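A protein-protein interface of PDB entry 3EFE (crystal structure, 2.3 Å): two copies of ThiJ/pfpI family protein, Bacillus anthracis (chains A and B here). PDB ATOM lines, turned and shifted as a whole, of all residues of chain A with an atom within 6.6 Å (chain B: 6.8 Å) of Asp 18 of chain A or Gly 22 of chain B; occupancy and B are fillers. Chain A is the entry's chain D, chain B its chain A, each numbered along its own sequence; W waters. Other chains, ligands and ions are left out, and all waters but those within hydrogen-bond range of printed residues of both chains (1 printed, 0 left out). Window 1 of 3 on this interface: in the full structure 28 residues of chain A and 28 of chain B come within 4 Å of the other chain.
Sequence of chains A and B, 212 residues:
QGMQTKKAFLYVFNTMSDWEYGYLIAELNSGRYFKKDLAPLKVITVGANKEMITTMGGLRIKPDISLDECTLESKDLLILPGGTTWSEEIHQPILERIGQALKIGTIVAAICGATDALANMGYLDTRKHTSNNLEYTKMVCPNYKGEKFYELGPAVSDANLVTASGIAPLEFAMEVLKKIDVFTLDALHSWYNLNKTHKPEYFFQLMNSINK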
ATOM      1  N   THR A  15      23.956  -3.151  35.328  1.00  0.00           N
ATOM      2  CA  THR A  15      22.661  -2.626  35.716  1.00  0.00           C
ATOM      3  C   THR A  15      22.662  -1.092  35.841  1.00  0.00           C
ATOM      4  O   THR A  15      21.628  -0.522  36.143  1.00  0.00           O
ATOM      5  CB  THR A  15      22.158  -3.272  37.090  1.00  0.00           C
ATOM      6  OG1 THR A  15      21.553  -4.581  36.851  1.00  0.00           O
ATOM      7  CG2 THR A  15      21.217  -2.416  37.760  1.00  0.00           C
ATOM      8  N   MET A  16      23.808  -0.408  35.628  1.00  0.00           N
ATOM      9  CA  MET A  16      23.796   1.068  35.844  1.00  0.00           C
ATOM     10  C   MET A  16      22.744   1.702  34.956  1.00  0.00           C
ATOM     11  O   MET A  16      22.536   1.320  33.793  1.00  0.00           O
ATOM     12  CB  MET A  16      25.168   1.710  35.703  1.00  0.00           C
ATOM     13  CG  MET A  16      25.955   1.495  34.376  1.00  0.00           C
ATOM     14  SD  MET A  16      27.576   2.184  34.338  1.00  0.00           S
ATOM     15  CE  MET A  16      27.269   3.558  35.058  1.00  0.00           C
ATOM     16  N   SER A  17      22.014   2.612  35.557  1.00  0.00           N
ATOM     17  CA  SER A  17      20.919   3.360  34.898  1.00  0.00           C
ATOM     18  C   SER A  17      21.421   4.472  33.928  1.00  0.00           C
ATOM     19  O   SER A  17      21.900   5.472  34.385  1.00  0.00           O
ATOM     20  CB  SER A  17      20.065   3.962  36.005  1.00  0.00           C
ATOM     21  OG  SER A  17      19.520   2.916  36.821  1.00  0.00           O
ATOM     22  N   ASP A  18      21.232   4.274  32.624  1.00  0.00           N
ATOM     23  CA  ASP A  18      21.788   5.091  31.541  1.00  0.00           C
ATOM     24  C   ASP A  18      21.353   6.537  31.525  1.00  0.00           C
ATOM     25  O   ASP A  18      22.142   7.432  31.155  1.00  0.00           O
ATOM     26  CB  ASP A  18      21.401   4.516  30.161  1.00  0.00           C
ATOM     27  CG  ASP A  18      21.847   3.040  29.985  1.00  0.00           C
ATOM     28  OD1 ASP A  18      22.694   2.736  29.134  1.00  0.00           O
ATOM     29  OD2 ASP A  18      21.340   2.204  30.718  1.00  0.00           O
ATOM     30  N   TRP A  19      20.118   6.782  31.938  1.00  0.00           N
ATOM     31  CA  TRP A  19      19.573   8.108  31.809  1.00  0.00           C
ATOM     32  C   TRP A  19      20.149   8.999  32.889  1.00  0.00           C
ATOM     33  O   TRP A  19      20.029  10.196  32.800  1.00  0.00           O
ATOM     34  CB  TRP A  19      18.060   8.091  31.802  1.00  0.00           C
ATOM     35  CG  TRP A  19      17.494   7.827  33.074  1.00  0.00           C
ATOM     36  CD1 TRP A  19      17.139   8.744  34.000  1.00  0.00           C
ATOM     37  CD2 TRP A  19      17.233   6.553  33.637  1.00  0.00           C
ATOM     38  NE1 TRP A  19      16.679   8.145  35.070  1.00  0.00           N
ATOM     39  CE2 TRP A  19      16.737   6.786  34.905  1.00  0.00           C
ATOM     40  CE3 TRP A  19      17.450   5.226  33.207  1.00  0.00           C
ATOM     41  CZ2 TRP A  19      16.371   5.760  35.770  1.00  0.00           C
ATOM     42  CZ3 TRP A  19      17.069   4.214  34.029  1.00  0.00           C
ATOM     43  CH2 TRP A  19      16.554   4.478  35.320  1.00  0.00           C
ATOM     44  N   GLU A  20      20.842   8.418  33.872  1.00  0.00           N
ATOM     45  CA  GLU A  20      21.112   9.150  35.124  1.00  0.00           C
ATOM     46  C   GLU A  20      22.448   9.931  35.025  1.00  0.00           C
ATOM     47  O   GLU A  20      22.596  10.995  35.635  1.00  0.00           O
ATOM     48  CB  GLU A  20      21.034   8.234  36.330  1.00  0.00           C
ATOM     49  CG  GLU A  20      19.607   7.924  36.674  1.00  0.00           C
ATOM     50  CD  GLU A  20      19.427   7.012  37.777  1.00  0.00           C
ATOM     51  OE1 GLU A  20      20.434   6.586  38.404  1.00  0.00           O
ATOM     52  OE2 GLU A  20      18.224   6.738  38.063  1.00  0.00           O
ATOM     53  N   TYR A  21      23.362   9.447  34.207  1.00  0.00           N
ATOM     54  CA  TYR A  21      24.731  10.038  34.071  1.00  0.00           C
ATOM     55  C   TYR A  21      25.003  10.639  32.717  1.00  0.00           C
ATOM     56  O   TYR A  21      25.993  11.289  32.591  1.00  0.00           O
ATOM     57  CB  TYR A  21      25.889   9.062  34.459  1.00  0.00           C
ATOM     58  CG  TYR A  21      25.783   7.819  33.702  1.00  0.00           C
ATOM     59  CD1 TYR A  21      26.177   7.762  32.369  1.00  0.00           C
ATOM     60  CD2 TYR A  21      25.118   6.698  34.248  1.00  0.00           C
ATOM     61  CE1 TYR A  21      25.963   6.620  31.633  1.00  0.00           C
ATOM     62  CE2 TYR A  21      24.941   5.578  33.510  1.00  0.00           C
ATOM     63  CZ  TYR A  21      25.370   5.531  32.235  1.00  0.00           C
ATOM     64  OH  TYR A  21      25.175   4.423  31.507  1.00  0.00           O
ATOM     65  N   GLY A  22      24.093  10.519  31.755  1.00  0.00           N
ATOM     66  CA  GLY A  22      24.369  10.858  30.363  1.00  0.00           C
ATOM     67  C   GLY A  22      24.707  12.309  30.029  1.00  0.00           C
ATOM     68  O   GLY A  22      25.632  12.569  29.302  1.00  0.00           O
ATOM     69  N   TYR A  23      23.880  13.223  30.516  1.00  0.00           N
ATOM     70  CA  TYR A  23      24.120  14.658  30.508  1.00  0.00           C
ATOM     71  C   TYR A  23      25.452  15.029  31.150  1.00  0.00           C
ATOM     72  O   TYR A  23      26.277  15.772  30.566  1.00  0.00           O
ATOM     73  CB  TYR A  23      23.015  15.353  31.295  1.00  0.00           C
ATOM     74  CG  TYR A  23      21.579  15.402  30.688  1.00  0.00           C
ATOM     75  CD1 TYR A  23      21.338  16.038  29.491  1.00  0.00           C
ATOM     76  CD2 TYR A  23      20.484  14.860  31.374  1.00  0.00           C
ATOM     77  CE1 TYR A  23      20.095  16.135  28.985  1.00  0.00           C
ATOM     78  CE2 TYR A  23      19.190  14.914  30.843  1.00  0.00           C
ATOM     79  CZ  TYR A  23      19.014  15.568  29.654  1.00  0.00           C
ATOM     80  OH  TYR A  23      17.774  15.679  29.086  1.00  0.00           O
ATOM     81  N   THR A  55      24.889  -2.097  30.882  1.00  0.00           N
ATOM     82  CA  THR A  55      24.008  -1.106  31.524  1.00  0.00           C
ATOM     83  C   THR A  55      22.611  -1.660  31.610  1.00  0.00           C
ATOM     84  O   THR A  55      22.356  -2.643  31.003  1.00  0.00           O
ATOM     85  CB  THR A  55      24.043   0.294  30.811  1.00  0.00           C
ATOM     86  OG1 THR A  55      23.462   0.191  29.527  1.00  0.00           O
ATOM     87  CG2 THR A  55      25.494   0.825  30.689  1.00  0.00           C
ATOM     88  N   MET A  56      21.714  -1.061  32.406  1.00  0.00           N
ATOM     89  CA  MET A  56      20.265  -1.326  32.297  1.00  0.00           C
ATOM     90  C   MET A  56      19.727  -1.235  30.897  1.00  0.00           C
ATOM     91  O   MET A  56      18.812  -1.965  30.576  1.00  0.00           O
ATOM     92  CB  MET A  56      19.443  -0.387  33.228  1.00  0.00           C
ATOM     93  CG  MET A  56      17.897  -0.722  33.382  1.00  0.00           C
ATOM     94  SD  MET A  56      17.116   0.526  34.370  1.00  0.00           S
ATOM     95  CE  MET A  56      15.438   0.134  34.095  1.00  0.00           C
ATOM     96  N   GLY A  57      20.259  -0.325  30.069  1.00  0.00           N
ATOM     97  CA  GLY A  57      19.875  -0.196  28.710  1.00  0.00           C
ATOM     98  C   GLY A  57      20.534  -1.228  27.804  1.00  0.00           C
ATOM     99  O   GLY A  57      20.195  -1.342  26.642  1.00  0.00           O
ATOM    100  N   GLY A  58      21.459  -2.022  28.318  1.00  0.00           N
ATOM    101  CA  GLY A  58      21.998  -3.150  27.555  1.00  0.00           C
ATOM    102  C   GLY A  58      23.304  -2.858  26.892  1.00  0.00           C
ATOM    103  O   GLY A  58      23.738  -3.610  26.056  1.00  0.00           O
ATOM    104  N   LEU A  59      23.960  -1.745  27.242  1.00  0.00           N
ATOM    105  CA  LEU A  59      25.204  -1.389  26.593  1.00  0.00           C
ATOM    106  C   LEU A  59      26.356  -2.116  27.258  1.00  0.00           C
ATOM    107  O   LEU A  59      26.503  -2.010  28.429  1.00  0.00           O
ATOM    108  CB  LEU A  59      25.400   0.101  26.675  1.00  0.00           C
ATOM    109  CG  LEU A  59      24.344   1.066  26.123  1.00  0.00           C
ATOM    110  CD1 LEU A  59      24.887   2.475  26.506  1.00  0.00           C
ATOM    111  CD2 LEU A  59      24.114   0.872  24.588  1.00  0.00           C
ATOM    112  N   ILE A  61      30.044  -2.318  28.292  1.00  0.00           N
ATOM    113  CA  ILE A  61      31.084  -1.341  28.441  1.00  0.00           C
ATOM    114  C   ILE A  61      32.339  -1.942  29.067  1.00  0.00           C
ATOM    115  O   ILE A  61      32.266  -2.692  30.020  1.00  0.00           O
ATOM    116  CB  ILE A  61      30.542  -0.138  29.320  1.00  0.00           C
ATOM    117  CG1 ILE A  61      29.406   0.563  28.553  1.00  0.00           C
ATOM    118  CG2 ILE A  61      31.685   0.807  29.784  1.00  0.00           C
ATOM    119  CD1 ILE A  61      28.566   1.557  29.425  1.00  0.00           C
ATOM    120  N   PRO A  81      26.204   6.340  39.658  1.00  0.00           N
ATOM    121  CA  PRO A  81      24.881   6.149  39.111  1.00  0.00           C
ATOM    122  C   PRO A  81      24.027   5.160  39.925  1.00  0.00           C
ATOM    123  O   PRO A  81      24.568   4.364  40.702  1.00  0.00           O
ATOM    124  CB  PRO A  81      25.143   5.560  37.728  1.00  0.00           C
ATOM    125  CG  PRO A  81      26.444   5.039  37.783  1.00  0.00           C
ATOM    126  CD  PRO A  81      27.213   5.606  38.921  1.00  0.00           C
ATOM    127  N   GLY A  82      22.705   5.272  39.765  1.00  0.00           N
ATOM    128  CA  GLY A  82      21.785   4.250  40.148  1.00  0.00           C
ATOM    129  C   GLY A  82      21.957   2.948  39.406  1.00  0.00           C
ATOM    130  O   GLY A  82      22.666   2.856  38.369  1.00  0.00           O
ATOM    131  N   SER B  17      25.816  10.688  21.578  1.00  0.00           N
ATOM    132  CA  SER B  17      25.400  11.594  22.640  1.00  0.00           C
ATOM    133  C   SER B  17      24.587  10.857  23.668  1.00  0.00           C
ATOM    134  O   SER B  17      23.389  10.569  23.454  1.00  0.00           O
ATOM    135  CB  SER B  17      24.601  12.769  22.085  1.00  0.00           C
ATOM    136  OG  SER B  17      25.390  13.603  21.230  1.00  0.00           O
ATOM    137  N   ASP B  18      25.262  10.603  24.809  1.00  0.00           N
ATOM    138  CA  ASP B  18      24.765   9.694  25.868  1.00  0.00           C
ATOM    139  C   ASP B  18      23.355   9.966  26.406  1.00  0.00           C
ATOM    140  O   ASP B  18      22.560   9.070  26.703  1.00  0.00           O
ATOM    141  CB  ASP B  18      25.767   9.740  27.028  1.00  0.00           C
ATOM    142  CG  ASP B  18      27.155   9.374  26.598  1.00  0.00           C
ATOM    143  OD1 ASP B  18      27.642   8.288  26.980  1.00  0.00           O
ATOM    144  OD2 ASP B  18      27.748  10.160  25.862  1.00  0.00           O
ATOM    145  N   TRP B  19      23.046  11.234  26.541  1.00  0.00           N
ATOM    146  CA  TRP B  19      21.784  11.617  27.167  1.00  0.00           C
ATOM    147  C   TRP B  19      20.537  11.435  26.256  1.00  0.00           C
ATOM    148  O   TRP B  19      19.404  11.602  26.686  1.00  0.00           O
ATOM    149  CB  TRP B  19      21.929  13.091  27.561  1.00  0.00           C
ATOM    150  CG  TRP B  19      21.888  14.011  26.430  1.00  0.00           C
ATOM    151  CD1 TRP B  19      20.762  14.541  25.866  1.00  0.00           C
ATOM    152  CD2 TRP B  19      22.985  14.527  25.700  1.00  0.00           C
ATOM    153  NE1 TRP B  19      21.099  15.355  24.830  1.00  0.00           N
ATOM    154  CE2 TRP B  19      22.459  15.375  24.706  1.00  0.00           C
ATOM    155  CE3 TRP B  19      24.379  14.397  25.808  1.00  0.00           C
ATOM    156  CZ2 TRP B  19      23.274  16.098  23.818  1.00  0.00           C
ATOM    157  CZ3 TRP B  19      25.171  15.099  24.940  1.00  0.00           C
ATOM    158  CH2 TRP B  19      24.620  15.923  23.932  1.00  0.00           C
ATOM    159  N   GLU B  20      20.777  11.190  24.974  1.00  0.00           N
ATOM    160  CA  GLU B  20      19.731  11.278  23.995  1.00  0.00           C
ATOM    161  C   GLU B  20      18.905   9.989  23.888  1.00  0.00           C
ATOM    162  O   GLU B  20      17.761  10.083  23.600  1.00  0.00           O
ATOM    163  CB  GLU B  20      20.330  11.683  22.639  1.00  0.00           C
ATOM    164  CG  GLU B  20      20.747  13.158  22.594  1.00  0.00           C
ATOM    165  CD  GLU B  20      21.254  13.580  21.254  1.00  0.00           C
ATOM    166  OE1 GLU B  20      21.325  12.706  20.333  1.00  0.00           O
ATOM    167  OE2 GLU B  20      21.640  14.785  21.139  1.00  0.00           O
ATOM    168  N   TYR B  21      19.509   8.834  24.146  1.00  0.00           N
ATOM    169  CA  TYR B  21      18.927   7.537  24.022  1.00  0.00           C
ATOM    170  C   TYR B  21      18.742   6.844  25.363  1.00  0.00           C
ATOM    171  O   TYR B  21      18.213   5.734  25.437  1.00  0.00           O
ATOM    172  CB  TYR B  21      19.804   6.678  23.163  1.00  0.00           C
ATOM    173  CG  TYR B  21      21.310   6.640  23.503  1.00  0.00           C
ATOM    174  CD1 TYR B  21      21.793   5.776  24.455  1.00  0.00           C
ATOM    175  CD2 TYR B  21      22.253   7.456  22.834  1.00  0.00           C
ATOM    176  CE1 TYR B  21      23.140   5.710  24.785  1.00  0.00           C
ATOM    177  CE2 TYR B  21      23.636   7.370  23.148  1.00  0.00           C
ATOM    178  CZ  TYR B  21      24.041   6.488  24.137  1.00  0.00           C
ATOM    179  OH  TYR B  21      25.336   6.325  24.543  1.00  0.00           O
ATOM    180  N   GLY B  22      19.193   7.489  26.420  1.00  0.00           N
ATOM    181  CA  GLY B  22      19.403   6.842  27.669  1.00  0.00           C
ATOM    182  C   GLY B  22      18.135   6.445  28.355  1.00  0.00           C
ATOM    183  O   GLY B  22      18.054   5.378  28.857  1.00  0.00           O
ATOM    184  N   TYR B  23      17.140   7.319  28.374  1.00  0.00           N
ATOM    185  CA  TYR B  23      15.846   6.946  28.892  1.00  0.00           C
ATOM    186  C   TYR B  23      15.199   5.830  28.087  1.00  0.00           C
ATOM    187  O   TYR B  23      14.674   4.890  28.662  1.00  0.00           O
ATOM    188  CB  TYR B  23      14.896   8.108  28.865  1.00  0.00           C
ATOM    189  CG  TYR B  23      15.163   9.268  29.766  1.00  0.00           C
ATOM    190  CD1 TYR B  23      14.774   9.254  31.100  1.00  0.00           C
ATOM    191  CD2 TYR B  23      15.681  10.460  29.234  1.00  0.00           C
ATOM    192  CE1 TYR B  23      14.949  10.415  31.889  1.00  0.00           C
ATOM    193  CE2 TYR B  23      15.907  11.575  29.996  1.00  0.00           C
ATOM    194  CZ  TYR B  23      15.519  11.566  31.307  1.00  0.00           C
ATOM    195  OH  TYR B  23      15.757  12.711  32.019  1.00  0.00           O
ATOM    196  N   LEU B  24      15.188   5.969  26.762  1.00  0.00           N
ATOM    197  CA  LEU B  24      14.647   4.966  25.838  1.00  0.00           C
ATOM    198  C   LEU B  24      15.229   3.567  26.011  1.00  0.00           C
ATOM    199  O   LEU B  24      14.527   2.606  26.239  1.00  0.00           O
ATOM    200  CB  LEU B  24      14.792   5.445  24.369  1.00  0.00           C
ATOM    201  CG  LEU B  24      13.948   4.725  23.325  1.00  0.00           C
ATOM    202  CD1 LEU B  24      12.506   4.346  23.865  1.00  0.00           C
ATOM    203  CD2 LEU B  24      13.864   5.496  22.026  1.00  0.00           C
ATOM    204  N   ILE B  25      16.532   3.443  25.909  1.00  0.00           N
ATOM    205  CA  ILE B  25      17.144   2.094  25.931  1.00  0.00           C
ATOM    206  C   ILE B  25      16.923   1.396  27.284  1.00  0.00           C
ATOM    207  O   ILE B  25      16.762   0.199  27.298  1.00  0.00           O
ATOM    208  CB  ILE B  25      18.609   2.074  25.386  1.00  0.00           C
ATOM    209  CG1 ILE B  25      19.624   2.817  26.243  1.00  0.00           C
ATOM    210  CG2 ILE B  25      18.649   2.652  23.919  1.00  0.00           C
ATOM    211  CD1 ILE B  25      21.005   2.359  26.067  1.00  0.00           C
ATOM    212  N   ALA B  26      16.870   2.143  28.395  1.00  0.00           N
ATOM    213  CA  ALA B  26      16.658   1.558  29.771  1.00  0.00           C
ATOM    214  C   ALA B  26      15.270   1.046  29.964  1.00  0.00           C
ATOM    215  O   ALA B  26      15.028  -0.089  30.463  1.00  0.00           O
ATOM    216  CB  ALA B  26      17.039   2.597  30.886  1.00  0.00           C
ATOM    217  N   GLU B  27      14.309   1.861  29.566  1.00  0.00           N
ATOM    218  CA  GLU B  27      12.924   1.440  29.586  1.00  0.00           C
ATOM    219  C   GLU B  27      12.652   0.189  28.776  1.00  0.00           C
ATOM    220  O   GLU B  27      11.816  -0.680  29.193  1.00  0.00           O
ATOM    221  CB  GLU B  27      11.968   2.568  29.166  1.00  0.00           C
ATOM    222  CG  GLU B  27      11.824   3.716  30.167  1.00  0.00           C
ATOM    223  CD  GLU B  27      11.824   3.319  31.678  1.00  0.00           C
ATOM    224  OE1 GLU B  27      11.252   2.278  32.110  1.00  0.00           O
ATOM    225  OE2 GLU B  27      12.367   4.128  32.471  1.00  0.00           O
ATOM    226  N   LEU B  59      32.371   6.575  27.217  1.00  0.00           N
ATOM    227  CA  LEU B  59      32.105   5.182  27.478  1.00  0.00           C
ATOM    228  C   LEU B  59      32.587   4.387  26.298  1.00  0.00           C
ATOM    229  O   LEU B  59      32.194   4.685  25.186  1.00  0.00           O
ATOM    230  CB  LEU B  59      30.618   4.915  27.695  1.00  0.00           C
ATOM    231  CG  LEU B  59      29.940   5.713  28.793  1.00  0.00           C
ATOM    232  CD1 LEU B  59      28.426   5.356  28.780  1.00  0.00           C
ATOM    233  CD2 LEU B  59      30.654   5.569  30.198  1.00  0.00           C
ATOM    234  N   PRO B 169      15.235  14.407  24.903  1.00  0.00           N
ATOM    235  CA  PRO B 169      15.225  12.936  25.024  1.00  0.00           C
ATOM    236  C   PRO B 169      13.987  12.267  25.647  1.00  0.00           C
ATOM    237  O   PRO B 169      13.752  11.105  25.389  1.00  0.00           O
ATOM    238  CB  PRO B 169      16.421  12.653  25.916  1.00  0.00           C
ATOM    239  CG  PRO B 169      16.694  13.913  26.585  1.00  0.00           C
ATOM    240  CD  PRO B 169      16.306  14.991  25.680  1.00  0.00           C
HETATM  241  O   HOH W   1      23.447   7.266  28.753  1.00  0.00           O
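The backbone carbonyl oxygen of Met 16 of chain A lies within hydrogen-bond range of the backbone NH of Met 56 of chain A, 2.9 Å away. The side-chain hydroxyl of Thr 55 of chain A lies close to the backbone NH of Gly 57 of chain A (3.3 Å). The side-chain hydroxyl of Thr 55 of chain A lies within hydrogen-bond range of the side-chain carboxylate of Asp 18 of chain A. The backbone NH (N) of Gly 57 of chain A lies within hydrogen-bond range of the side-chain carboxylate (OD2) of Asp 18 of chain A, at 2.8 Å. OG1 of Thr 55 of chain A lies within hydrogen-bond range of N of Leu 59 of chain A (3.0 Å).
Gly 22 of chain B touches Asp 18 of chain A (O to CB, 3.7 Å). Ile 25 of chain B touches Asp 18 of chain A (CD1 to OD1, 3.5 Å). Gly 22 of chain B touches Trp 19 of chain A (C to CB, 3.8 Å). Trp 19 of chain A touches Ala 26 of chain B. Leu 59 of chain B touches Tyr 21 of chain A. Gly 22 of chain A touches Asp 18 of chain B. Tyr 23 of chain A touches Pro 169 of chain B (OH to CG, 3.2 Å). CA of Ala 26 of chain B touches CA of Gly 57 of chain A, 3.8 Å away. CD1 of Ile 25 of chain B touches CG of Leu 59 of chain A (3.6 Å). Leu 59 of chain B touches Ile 61 of chain A (CD1 to CD1, 3.9 Å).
Asp 18 of chain A touches just these residues of chain B: Gly 22 (3.7 Å) and Ile 25 (3.5 Å). Of the printed residues of chain B, Ile 61 of chain A touches Leu 59. Printed residues of chain B within 4 Å of Tyr 23 of chain A: Trp 19 (3.5 Å) and Pro 169 (3.2 Å). Tyr 21 of chain B touches none of the printed residues of chain A. Glu 20 of chain B touches none of the printed residues of chain A.
Printed residues of chain B that touch a printed residue of chain A: Asp 18, Trp 19, Gly 22, Tyr 23, Ile 25, Ala 26, Leu 59 and Pro 169. Hydrophobic or aromatic side chains of chain B that line the printed part of chain A: Trp 19, Tyr 23, Ile 25, Ala 26, Leu 59 and Pro 169. Of the 17 printed residues of chain A, 9 touch a printed residue of chain B. Among the printed residues, 15 pairs touch across the chains.
Asp 18 of chain A touches Gly 22 of chain B, and with the chains exchanged Gly 22 of chain A touches Asp 18 of chain B. Trp 19 of chain A touches Gly 22 of chain B, and with the chains exchanged Gly 22 of chain A touches Trp 19 of chain B. Trp 19 of chain A touches Tyr 23 of chain B, and with the chains exchanged Tyr 23 of chain A touches Trp 19 of chain B. Tyr 21 of chain A touches Leu 59 of chain B, but with the chains exchanged Leu 59 of chain A does not touch Tyr 21 of chain B (4.1 Å). Positions printed for both chains: 17, 18, 19, 20, 21, 22, 23 and 59. Of the 15 pairs that touch across the chains among the printed residues, 6 have their exchanged pair printed and touching as well.
Water W1 lies within hydrogen-bond range of O of Asp 18 of chain A (2.7 Å) and O of Asp 18 of chain B (2.9 Å).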
